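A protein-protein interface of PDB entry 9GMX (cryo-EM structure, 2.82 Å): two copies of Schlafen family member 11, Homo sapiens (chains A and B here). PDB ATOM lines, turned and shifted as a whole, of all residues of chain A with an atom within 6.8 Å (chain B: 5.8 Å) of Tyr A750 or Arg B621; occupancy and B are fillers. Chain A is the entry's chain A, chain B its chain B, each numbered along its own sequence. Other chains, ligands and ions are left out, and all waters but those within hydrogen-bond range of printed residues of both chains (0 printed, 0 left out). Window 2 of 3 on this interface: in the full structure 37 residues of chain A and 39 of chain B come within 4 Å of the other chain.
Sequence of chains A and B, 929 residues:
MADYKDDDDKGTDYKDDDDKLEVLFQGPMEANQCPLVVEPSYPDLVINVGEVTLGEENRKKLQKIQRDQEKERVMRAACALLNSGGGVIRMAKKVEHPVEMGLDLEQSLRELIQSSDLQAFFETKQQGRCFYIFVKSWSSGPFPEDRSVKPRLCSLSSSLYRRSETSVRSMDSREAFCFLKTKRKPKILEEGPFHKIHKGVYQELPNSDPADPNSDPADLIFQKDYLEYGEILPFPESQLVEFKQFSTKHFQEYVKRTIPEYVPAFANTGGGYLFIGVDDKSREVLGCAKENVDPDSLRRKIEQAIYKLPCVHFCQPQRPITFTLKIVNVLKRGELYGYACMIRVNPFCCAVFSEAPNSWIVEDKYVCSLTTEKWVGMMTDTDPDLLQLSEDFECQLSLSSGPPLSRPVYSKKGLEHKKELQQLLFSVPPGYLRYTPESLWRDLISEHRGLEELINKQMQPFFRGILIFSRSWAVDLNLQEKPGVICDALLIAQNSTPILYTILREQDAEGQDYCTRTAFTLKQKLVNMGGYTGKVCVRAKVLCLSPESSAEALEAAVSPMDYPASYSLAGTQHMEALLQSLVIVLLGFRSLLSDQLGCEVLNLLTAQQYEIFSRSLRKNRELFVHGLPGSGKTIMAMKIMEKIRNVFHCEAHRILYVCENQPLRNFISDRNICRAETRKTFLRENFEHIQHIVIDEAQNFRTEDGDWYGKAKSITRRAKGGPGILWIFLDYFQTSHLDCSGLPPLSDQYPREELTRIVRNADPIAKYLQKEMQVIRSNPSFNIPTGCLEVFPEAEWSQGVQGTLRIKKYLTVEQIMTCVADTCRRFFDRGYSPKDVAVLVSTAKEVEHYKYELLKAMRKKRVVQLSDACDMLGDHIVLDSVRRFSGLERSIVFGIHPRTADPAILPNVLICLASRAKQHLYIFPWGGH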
ATOM      1  N   ASN A 620      -5.876 -25.526  -2.535  1.00  0.00           N
ATOM      2  CA  ASN A 620      -7.248 -25.082  -2.351  1.00  0.00           C
ATOM      3  C   ASN A 620      -8.023 -26.192  -1.666  1.00  0.00           C
ATOM      4  O   ASN A 620      -7.625 -27.358  -1.670  1.00  0.00           O
ATOM      5  CB  ASN A 620      -7.932 -24.763  -3.680  1.00  0.00           C
ATOM      6  CG  ASN A 620      -7.234 -23.672  -4.440  1.00  0.00           C
ATOM      7  OD1 ASN A 620      -7.592 -22.505  -4.335  1.00  0.00           O
ATOM      8  ND2 ASN A 620      -6.223 -24.042  -5.208  1.00  0.00           N
ATOM      9  N   GLU A 622     -11.870 -25.211  -1.128  1.00  0.00           N
ATOM     10  CA  GLU A 622     -13.001 -24.794  -1.936  1.00  0.00           C
ATOM     11  C   GLU A 622     -12.474 -24.156  -3.211  1.00  0.00           C
ATOM     12  O   GLU A 622     -11.598 -23.294  -3.169  1.00  0.00           O
ATOM     13  CB  GLU A 622     -13.949 -23.830  -1.229  1.00  0.00           C
ATOM     14  CG  GLU A 622     -14.540 -24.367   0.052  1.00  0.00           C
ATOM     15  CD  GLU A 622     -15.336 -23.320   0.797  1.00  0.00           C
ATOM     16  OE1 GLU A 622     -16.503 -23.594   1.145  1.00  0.00           O
ATOM     17  OE2 GLU A 622     -14.795 -22.218   1.030  1.00  0.00           O
ATOM     18  N   LEU A 623     -13.009 -24.589  -4.347  1.00  0.00           N
ATOM     19  CA  LEU A 623     -12.567 -24.085  -5.635  1.00  0.00           C
ATOM     20  C   LEU A 623     -13.752 -24.047  -6.584  1.00  0.00           C
ATOM     21  O   LEU A 623     -14.559 -24.976  -6.618  1.00  0.00           O
ATOM     22  CB  LEU A 623     -11.436 -24.955  -6.200  1.00  0.00           C
ATOM     23  CG  LEU A 623     -10.733 -24.509  -7.482  1.00  0.00           C
ATOM     24  CD1 LEU A 623     -10.020 -23.209  -7.295  1.00  0.00           C
ATOM     25  CD2 LEU A 623      -9.753 -25.567  -7.894  1.00  0.00           C
ATOM     26  N   PHE A 624     -13.861 -22.959  -7.331  1.00  0.00           N
ATOM     27  CA  PHE A 624     -14.842 -22.822  -8.393  1.00  0.00           C
ATOM     28  C   PHE A 624     -14.105 -22.901  -9.716  1.00  0.00           C
ATOM     29  O   PHE A 624     -13.341 -21.995 -10.057  1.00  0.00           O
ATOM     30  CB  PHE A 624     -15.601 -21.506  -8.279  1.00  0.00           C
ATOM     31  CG  PHE A 624     -16.449 -21.407  -7.056  1.00  0.00           C
ATOM     32  CD1 PHE A 624     -15.911 -20.986  -5.858  1.00  0.00           C
ATOM     33  CD2 PHE A 624     -17.783 -21.743  -7.100  1.00  0.00           C
ATOM     34  CE1 PHE A 624     -16.687 -20.902  -4.733  1.00  0.00           C
ATOM     35  CE2 PHE A 624     -18.562 -21.659  -5.979  1.00  0.00           C
ATOM     36  CZ  PHE A 624     -18.015 -21.240  -4.794  1.00  0.00           C
ATOM     37  N   TYR A 709     -25.783 -25.984  -2.336  1.00  0.00           N
ATOM     38  CA  TYR A 709     -24.490 -25.402  -2.000  1.00  0.00           C
ATOM     39  C   TYR A 709     -24.273 -25.382  -0.494  1.00  0.00           C
ATOM     40  O   TYR A 709     -23.181 -25.707  -0.010  1.00  0.00           O
ATOM     41  CB  TYR A 709     -24.386 -23.997  -2.583  1.00  0.00           C
ATOM     42  CG  TYR A 709     -23.065 -23.321  -2.322  1.00  0.00           C
ATOM     43  CD1 TYR A 709     -21.879 -24.039  -2.353  1.00  0.00           C
ATOM     44  CD2 TYR A 709     -22.999 -21.965  -2.061  1.00  0.00           C
ATOM     45  CE1 TYR A 709     -20.678 -23.431  -2.118  1.00  0.00           C
ATOM     46  CE2 TYR A 709     -21.798 -21.348  -1.830  1.00  0.00           C
ATOM     47  CZ  TYR A 709     -20.640 -22.084  -1.861  1.00  0.00           C
ATOM     48  OH  TYR A 709     -19.432 -21.470  -1.629  1.00  0.00           O
ATOM     49  N   PRO A 744     -23.324 -19.471  -5.326  1.00  0.00           N
ATOM     50  CA  PRO A 744     -23.041 -18.197  -4.687  1.00  0.00           C
ATOM     51  C   PRO A 744     -22.795 -17.127  -5.733  1.00  0.00           C
ATOM     52  O   PRO A 744     -22.486 -17.442  -6.889  1.00  0.00           O
ATOM     53  CB  PRO A 744     -21.776 -18.486  -3.870  1.00  0.00           C
ATOM     54  CG  PRO A 744     -21.139 -19.598  -4.563  1.00  0.00           C
ATOM     55  CD  PRO A 744     -22.234 -20.436  -5.120  1.00  0.00           C
ATOM     56  N   PRO A 745     -22.926 -15.855  -5.373  1.00  0.00           N
ATOM     57  CA  PRO A 745     -22.754 -14.793  -6.369  1.00  0.00           C
ATOM     58  C   PRO A 745     -21.360 -14.827  -6.976  1.00  0.00           C
ATOM     59  O   PRO A 745     -20.397 -15.271  -6.350  1.00  0.00           O
ATOM     60  CB  PRO A 745     -22.994 -13.501  -5.581  1.00  0.00           C
ATOM     61  CG  PRO A 745     -23.310 -13.885  -4.195  1.00  0.00           C
ATOM     62  CD  PRO A 745     -23.162 -15.347  -4.015  1.00  0.00           C
ATOM     63  N   LEU A 746     -21.265 -14.348  -8.215  1.00  0.00           N
ATOM     64  CA  LEU A 746     -19.994 -14.383  -8.925  1.00  0.00           C
ATOM     65  C   LEU A 746     -18.873 -13.756  -8.106  1.00  0.00           C
ATOM     66  O   LEU A 746     -17.742 -14.249  -8.124  1.00  0.00           O
ATOM     67  CB  LEU A 746     -20.136 -13.671 -10.270  1.00  0.00           C
ATOM     68  CG  LEU A 746     -18.881 -13.582 -11.135  1.00  0.00           C
ATOM     69  CD1 LEU A 746     -18.398 -14.965 -11.530  1.00  0.00           C
ATOM     70  CD2 LEU A 746     -19.157 -12.730 -12.360  1.00  0.00           C
ATOM     71  N   SER A 747     -19.163 -12.677  -7.383  1.00  0.00           N
ATOM     72  CA  SER A 747     -18.146 -12.047  -6.553  1.00  0.00           C
ATOM     73  C   SER A 747     -17.672 -12.959  -5.433  1.00  0.00           C
ATOM     74  O   SER A 747     -16.584 -12.742  -4.892  1.00  0.00           O
ATOM     75  CB  SER A 747     -18.692 -10.747  -5.967  1.00  0.00           C
ATOM     76  OG  SER A 747     -19.959 -10.956  -5.368  1.00  0.00           O
ATOM     77  N   ASP A 748     -18.459 -13.969  -5.078  1.00  0.00           N
ATOM     78  CA  ASP A 748     -18.130 -14.887  -4.001  1.00  0.00           C
ATOM     79  C   ASP A 748     -17.385 -16.113  -4.506  1.00  0.00           C
ATOM     80  O   ASP A 748     -16.639 -16.726  -3.738  1.00  0.00           O
ATOM     81  CB  ASP A 748     -19.433 -15.277  -3.271  1.00  0.00           C
ATOM     82  CG  ASP A 748     -19.300 -16.482  -2.325  1.00  0.00           C
ATOM     83  OD1 ASP A 748     -18.327 -17.257  -2.365  1.00  0.00           O
ATOM     84  OD2 ASP A 748     -20.234 -16.661  -1.514  1.00  0.00           O
ATOM     85  N   GLN A 749     -17.502 -16.438  -5.789  1.00  0.00           N
ATOM     86  CA  GLN A 749     -16.975 -17.696  -6.299  1.00  0.00           C
ATOM     87  C   GLN A 749     -15.453 -17.690  -6.384  1.00  0.00           C
ATOM     88  O   GLN A 749     -14.896 -17.622  -7.484  1.00  0.00           O
ATOM     89  CB  GLN A 749     -17.567 -17.986  -7.675  1.00  0.00           C
ATOM     90  CG  GLN A 749     -19.030 -18.394  -7.660  1.00  0.00           C
ATOM     91  CD  GLN A 749     -19.644 -18.383  -9.038  1.00  0.00           C
ATOM     92  OE1 GLN A 749     -18.940 -18.355 -10.040  1.00  0.00           O
ATOM     93  NE2 GLN A 749     -20.962 -18.403  -9.094  1.00  0.00           N
ATOM     94  N   TYR A 750     -14.778 -17.773  -5.240  1.00  0.00           N
ATOM     95  CA  TYR A 750     -13.326 -17.806  -5.156  1.00  0.00           C
ATOM     96  C   TYR A 750     -12.910 -18.792  -4.075  1.00  0.00           C
ATOM     97  O   TYR A 750     -13.675 -19.045  -3.139  1.00  0.00           O
ATOM     98  CB  TYR A 750     -12.746 -16.425  -4.831  1.00  0.00           C
ATOM     99  CG  TYR A 750     -12.835 -15.443  -5.964  1.00  0.00           C
ATOM    100  CD1 TYR A 750     -11.880 -15.410  -6.960  1.00  0.00           C
ATOM    101  CD2 TYR A 750     -13.890 -14.555  -6.043  1.00  0.00           C
ATOM    102  CE1 TYR A 750     -11.968 -14.513  -7.993  1.00  0.00           C
ATOM    103  CE2 TYR A 750     -13.987 -13.658  -7.071  1.00  0.00           C
ATOM    104  CZ  TYR A 750     -13.029 -13.640  -8.043  1.00  0.00           C
ATOM    105  OH  TYR A 750     -13.140 -12.734  -9.070  1.00  0.00           O
ATOM    106  N   PRO A 751     -11.711 -19.372  -4.179  1.00  0.00           N
ATOM    107  CA  PRO A 751     -10.719 -19.219  -5.245  1.00  0.00           C
ATOM    108  C   PRO A 751     -11.200 -19.832  -6.550  1.00  0.00           C
ATOM    109  O   PRO A 751     -12.021 -20.736  -6.555  1.00  0.00           O
ATOM    110  CB  PRO A 751      -9.495 -19.943  -4.680  1.00  0.00           C
ATOM    111  CG  PRO A 751     -10.056 -20.971  -3.779  1.00  0.00           C
ATOM    112  CD  PRO A 751     -11.258 -20.326  -3.157  1.00  0.00           C
ATOM    113  N   ARG A 752     -10.700 -19.351  -7.677  1.00  0.00           N
ATOM    114  CA  ARG A 752     -11.247 -19.689  -8.977  1.00  0.00           C
ATOM    115  C   ARG A 752     -10.162 -20.233  -9.887  1.00  0.00           C
ATOM    116  O   ARG A 752      -9.075 -19.664  -9.985  1.00  0.00           O
ATOM    117  CB  ARG A 752     -11.874 -18.466  -9.616  1.00  0.00           C
ATOM    118  CG  ARG A 752     -12.742 -18.765 -10.801  1.00  0.00           C
ATOM    119  CD  ARG A 752     -13.454 -17.520 -11.247  1.00  0.00           C
ATOM    120  NE  ARG A 752     -14.301 -16.994 -10.189  1.00  0.00           N
ATOM    121  CZ  ARG A 752     -14.882 -15.805 -10.218  1.00  0.00           C
ATOM    122  NH1 ARG A 752     -14.711 -14.977 -11.234  1.00  0.00           N
ATOM    123  NH2 ARG A 752     -15.651 -15.435  -9.201  1.00  0.00           N
ATOM    124  N   SER B 616      -1.563 -15.891  -9.295  1.00  0.00           N
ATOM    125  CA  SER B 616      -2.606 -16.208  -8.332  1.00  0.00           C
ATOM    126  C   SER B 616      -3.445 -15.003  -7.945  1.00  0.00           C
ATOM    127  O   SER B 616      -4.415 -15.169  -7.203  1.00  0.00           O
ATOM    128  CB  SER B 616      -1.989 -16.810  -7.075  1.00  0.00           C
ATOM    129  OG  SER B 616      -1.362 -18.041  -7.363  1.00  0.00           O
ATOM    130  N   LEU B 617      -3.101 -13.804  -8.404  1.00  0.00           N
ATOM    131  CA  LEU B 617      -3.888 -12.633  -8.036  1.00  0.00           C
ATOM    132  C   LEU B 617      -5.285 -12.710  -8.634  1.00  0.00           C
ATOM    133  O   LEU B 617      -6.280 -12.421  -7.962  1.00  0.00           O
ATOM    134  CB  LEU B 617      -3.183 -11.360  -8.491  1.00  0.00           C
ATOM    135  CG  LEU B 617      -3.922 -10.070  -8.132  1.00  0.00           C
ATOM    136  CD1 LEU B 617      -3.951  -9.892  -6.629  1.00  0.00           C
ATOM    137  CD2 LEU B 617      -3.280  -8.875  -8.792  1.00  0.00           C
ATOM    138  N   ARG B 618      -5.373 -13.084  -9.908  1.00  0.00           N
ATOM    139  CA  ARG B 618      -6.663 -13.200 -10.574  1.00  0.00           C
ATOM    140  C   ARG B 618      -7.467 -14.388 -10.070  1.00  0.00           C
ATOM    141  O   ARG B 618      -8.682 -14.440 -10.282  1.00  0.00           O
ATOM    142  CB  ARG B 618      -6.440 -13.311 -12.079  1.00  0.00           C
ATOM    143  CG  ARG B 618      -7.687 -13.177 -12.916  1.00  0.00           C
ATOM    144  CD  ARG B 618      -7.570 -13.980 -14.208  1.00  0.00           C
ATOM    145  NE  ARG B 618      -8.338 -13.388 -15.297  1.00  0.00           N
ATOM    146  CZ  ARG B 618      -8.137 -12.172 -15.786  1.00  0.00           C
ATOM    147  NH1 ARG B 618      -7.163 -11.396 -15.338  1.00  0.00           N
ATOM    148  NH2 ARG B 618      -8.927 -11.725 -16.757  1.00  0.00           N
ATOM    149  N   LYS B 619      -6.823 -15.331  -9.395  1.00  0.00           N
ATOM    150  CA  LYS B 619      -7.474 -16.558  -8.981  1.00  0.00           C
ATOM    151  C   LYS B 619      -7.918 -16.536  -7.530  1.00  0.00           C
ATOM    152  O   LYS B 619      -8.649 -17.438  -7.113  1.00  0.00           O
ATOM    153  CB  LYS B 619      -6.523 -17.731  -9.189  1.00  0.00           C
ATOM    154  CG  LYS B 619      -5.849 -17.710 -10.539  1.00  0.00           C
ATOM    155  CD  LYS B 619      -5.445 -19.096 -10.991  1.00  0.00           C
ATOM    156  CE  LYS B 619      -4.522 -19.764 -10.009  1.00  0.00           C
ATOM    157  NZ  LYS B 619      -3.983 -21.022 -10.572  1.00  0.00           N
ATOM    158  N   ASN B 620      -7.502 -15.540  -6.752  1.00  0.00           N
ATOM    159  CA  ASN B 620      -7.756 -15.517  -5.320  1.00  0.00           C
ATOM    160  C   ASN B 620      -8.166 -14.119  -4.893  1.00  0.00           C
ATOM    161  O   ASN B 620      -7.880 -13.127  -5.564  1.00  0.00           O
ATOM    162  CB  ASN B 620      -6.531 -15.953  -4.517  1.00  0.00           C
ATOM    163  CG  ASN B 620      -6.192 -17.406  -4.707  1.00  0.00           C
ATOM    164  OD1 ASN B 620      -6.752 -18.270  -4.049  1.00  0.00           O
ATOM    165  ND2 ASN B 620      -5.258 -17.685  -5.598  1.00  0.00           N
ATOM    166  N   ARG B 621      -8.875 -14.063  -3.769  1.00  0.00           N
ATOM    167  CA  ARG B 621      -9.093 -12.821  -3.045  1.00  0.00           C
ATOM    168  C   ARG B 621      -8.467 -12.952  -1.666  1.00  0.00           C
ATOM    169  O   ARG B 621      -7.635 -12.134  -1.270  1.00  0.00           O
ATOM    170  CB  ARG B 621     -10.585 -12.510  -2.933  1.00  0.00           C
ATOM    171  CG  ARG B 621     -11.244 -12.105  -4.232  1.00  0.00           C
ATOM    172  CD  ARG B 621     -10.679 -10.804  -4.761  1.00  0.00           C
ATOM    173  NE  ARG B 621     -11.400 -10.316  -5.931  1.00  0.00           N
ATOM    174  CZ  ARG B 621     -11.050 -10.545  -7.189  1.00  0.00           C
ATOM    175  NH1 ARG B 621     -10.001 -11.292  -7.493  1.00  0.00           N
ATOM    176  NH2 ARG B 621     -11.769 -10.007  -8.168  1.00  0.00           N
ATOM    177  N   GLU B 622      -8.867 -13.987  -0.935  1.00  0.00           N
ATOM    178  CA  GLU B 622      -8.191 -14.351   0.298  1.00  0.00           C
ATOM    179  C   GLU B 622      -7.084 -15.350  -0.001  1.00  0.00           C
ATOM    180  O   GLU B 622      -7.312 -16.370  -0.650  1.00  0.00           O
ATOM    181  CB  GLU B 622      -9.185 -14.959   1.283  1.00  0.00           C
ATOM    182  CG  GLU B 622      -8.614 -15.318   2.643  1.00  0.00           C
ATOM    183  CD  GLU B 622      -9.647 -15.873   3.607  1.00  0.00           C
ATOM    184  OE1 GLU B 622     -10.819 -16.017   3.198  1.00  0.00           O
ATOM    185  OE2 GLU B 622      -9.291 -16.192   4.758  1.00  0.00           O
ATOM    186  N   LEU B 623      -5.878 -15.059   0.476  1.00  0.00           N
ATOM    187  CA  LEU B 623      -4.747 -15.945   0.258  1.00  0.00           C
ATOM    188  C   LEU B 623      -3.817 -15.883   1.456  1.00  0.00           C
ATOM    189  O   LEU B 623      -3.524 -14.804   1.968  1.00  0.00           O
ATOM    190  CB  LEU B 623      -3.996 -15.579  -1.029  1.00  0.00           C
ATOM    191  CG  LEU B 623      -2.892 -16.534  -1.481  1.00  0.00           C
ATOM    192  CD1 LEU B 623      -3.435 -17.894  -1.797  1.00  0.00           C
ATOM    193  CD2 LEU B 623      -2.200 -15.977  -2.693  1.00  0.00           C
ATOM    194  N   PHE B 648      -6.452  -3.553 -10.665  1.00  0.00           N
ATOM    195  CA  PHE B 648      -7.726  -3.049 -10.179  1.00  0.00           C
ATOM    196  C   PHE B 648      -7.888  -1.553 -10.390  1.00  0.00           C
ATOM    197  O   PHE B 648      -8.953  -1.014 -10.076  1.00  0.00           O
ATOM    198  CB  PHE B 648      -7.874  -3.382  -8.693  1.00  0.00           C
ATOM    199  CG  PHE B 648      -7.999  -4.853  -8.415  1.00  0.00           C
ATOM    200  CD1 PHE B 648      -6.936  -5.706  -8.639  1.00  0.00           C
ATOM    201  CD2 PHE B 648      -9.165  -5.375  -7.893  1.00  0.00           C
ATOM    202  CE1 PHE B 648      -7.045  -7.052  -8.377  1.00  0.00           C
ATOM    203  CE2 PHE B 648      -9.275  -6.721  -7.625  1.00  0.00           C
ATOM    204  CZ  PHE B 648      -8.211  -7.558  -7.864  1.00  0.00           C
ATOM    205  N   GLY B 721     -16.051  -3.461  -5.411  1.00  0.00           N
ATOM    206  CA  GLY B 721     -15.869  -4.429  -6.474  1.00  0.00           C
ATOM    207  C   GLY B 721     -15.788  -5.844  -5.944  1.00  0.00           C
ATOM    208  O   GLY B 721     -14.786  -6.536  -6.149  1.00  0.00           O
ATOM    209  N   PRO B 723     -15.606  -8.612  -2.757  1.00  0.00           N
ATOM    210  CA  PRO B 723     -14.568  -8.617  -1.723  1.00  0.00           C
ATOM    211  C   PRO B 723     -13.235  -8.186  -2.312  1.00  0.00           C
ATOM    212  O   PRO B 723     -12.897  -8.529  -3.445  1.00  0.00           O
ATOM    213  CB  PRO B 723     -14.537 -10.076  -1.250  1.00  0.00           C
ATOM    214  CG  PRO B 723     -15.105 -10.857  -2.373  1.00  0.00           C
ATOM    215  CD  PRO B 723     -16.124  -9.963  -3.022  1.00  0.00           C
ATOM    216  N   GLY B 724     -12.483  -7.413  -1.533  1.00  0.00           N
ATOM    217  CA  GLY B 724     -11.166  -6.988  -1.942  1.00  0.00           C
ATOM    218  C   GLY B 724     -10.112  -8.038  -1.660  1.00  0.00           C
ATOM    219  O   GLY B 724     -10.383  -9.132  -1.169  1.00  0.00           O
ATOM    220  N   ILE B 725      -8.871  -7.680  -1.985  1.00  0.00           N
ATOM    221  CA  ILE B 725      -7.743  -8.570  -1.764  1.00  0.00           C
ATOM    222  C   ILE B 725      -7.402  -8.587  -0.283  1.00  0.00           C
ATOM    223  O   ILE B 725      -7.276  -7.534   0.352  1.00  0.00           O
ATOM    224  CB  ILE B 725      -6.537  -8.116  -2.599  1.00  0.00           C
ATOM    225  CG1 ILE B 725      -6.847  -8.179  -4.096  1.00  0.00           C
ATOM    226  CG2 ILE B 725      -5.325  -8.956  -2.280  1.00  0.00           C
ATOM    227  CD1 ILE B 725      -7.019  -9.569  -4.644  1.00  0.00           C
ATOM    228  N   LEU B 726      -7.258  -9.783   0.279  1.00  0.00           N
ATOM    229  CA  LEU B 726      -6.765  -9.953   1.643  1.00  0.00           C
ATOM    230  C   LEU B 726      -5.700 -11.036   1.562  1.00  0.00           C
ATOM    231  O   LEU B 726      -6.014 -12.226   1.589  1.00  0.00           O
ATOM    232  CB  LEU B 726      -7.878 -10.320   2.618  1.00  0.00           C
ATOM    233  CG  LEU B 726      -7.472 -10.673   4.054  1.00  0.00           C
ATOM    234  CD1 LEU B 726      -6.940 -12.088   4.179  1.00  0.00           C
ATOM    235  CD2 LEU B 726      -6.440  -9.686   4.570  1.00  0.00           C
ATOM    236  N   TRP B 727      -4.443 -10.622   1.459  1.00  0.00           N
ATOM    237  CA  TRP B 727      -3.320 -11.543   1.381  1.00  0.00           C
ATOM    238  C   TRP B 727      -2.481 -11.408   2.639  1.00  0.00           C
ATOM    239  O   TRP B 727      -2.034 -10.309   2.973  1.00  0.00           O
ATOM    240  CB  TRP B 727      -2.485 -11.268   0.135  1.00  0.00           C
ATOM    241  CG  TRP B 727      -3.083 -11.858  -1.092  1.00  0.00           C
ATOM    242  CD1 TRP B 727      -4.400 -12.102  -1.322  1.00  0.00           C
ATOM    243  CD2 TRP B 727      -2.383 -12.306  -2.252  1.00  0.00           C
ATOM    244  NE1 TRP B 727      -4.570 -12.663  -2.558  1.00  0.00           N
ATOM    245  CE2 TRP B 727      -3.344 -12.801  -3.150  1.00  0.00           C
ATOM    246  CE3 TRP B 727      -1.039 -12.337  -2.619  1.00  0.00           C
ATOM    247  CZ2 TRP B 727      -3.003 -13.315  -4.390  1.00  0.00           C
ATOM    248  CZ3 TRP B 727      -0.707 -12.845  -3.846  1.00  0.00           C
ATOM    249  CH2 TRP B 727      -1.681 -13.329  -4.719  1.00  0.00           C
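The side-chain hydroxyl of Tyr A750 is in hydrogen-bond range of the guanidinium group of Arg B621 (3.2 Å). The backbone NH (N) of Arg A752 is in hydrogen-bond range of the backbone carbonyl oxygen (O) of Lys B619, at 2.9 Å.
3 positions are printed for both chains. Of the 6 pairs that touch across the chains among the printed residues, none has its exchanged pair printed and touching as well.
Of the 14 printed residues of chain A, 4 touch a printed residue of chain B. Along chain A the printed residues that touch a printed residue of chain B span positions 747 to 752.
Of the printed residues of chain B, Ser A747 touches Pro B723 (3.4 Å). Of chain A, only Tyr A750 comes within 4 Å of Arg B621. Of the printed residues of chain A, Pro B723 touches Ser A747 (3.4 Å). The nearest residue of chain A that does not touch Arg B621 is Ser A747 (5.4 Å).
Among the printed residues, pairs that only touch across the chains: Ser A747 with Pro B723 (3.4 Å), Tyr A750 with Lys B619 (3.8 Å), Pro A751 with Lys B619 (3.3 Å) and Pro A751 with Asn B620 (3.3 Å).
The backbone carbonyl oxygen (O) of Arg B621 lies close to the indole nitrogen (NE1) of Trp B727, at 3.4 Å. The guanidinium group of Arg A752 lies within hydrogen-bond range of the backbone carbonyl oxygen of Gln A749 (2.8 Å). The backbone NH (N) of Phe A624 is in hydrogen-bond range of the backbone carbonyl oxygen (O) of Pro A751 (3.0 Å). OH of Tyr A750 lies within hydrogen-bond range of NH1 of Arg A752, 3.5 Å away. The backbone carbonyl oxygen (O) of Leu A746 sits at hydrogen-bond distance from the guanidinium group (NH2) of Arg A752 (2.6 Å). O of Ser B616 sits at hydrogen-bond distance from ND2 of Asn B620 (3.1 Å).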
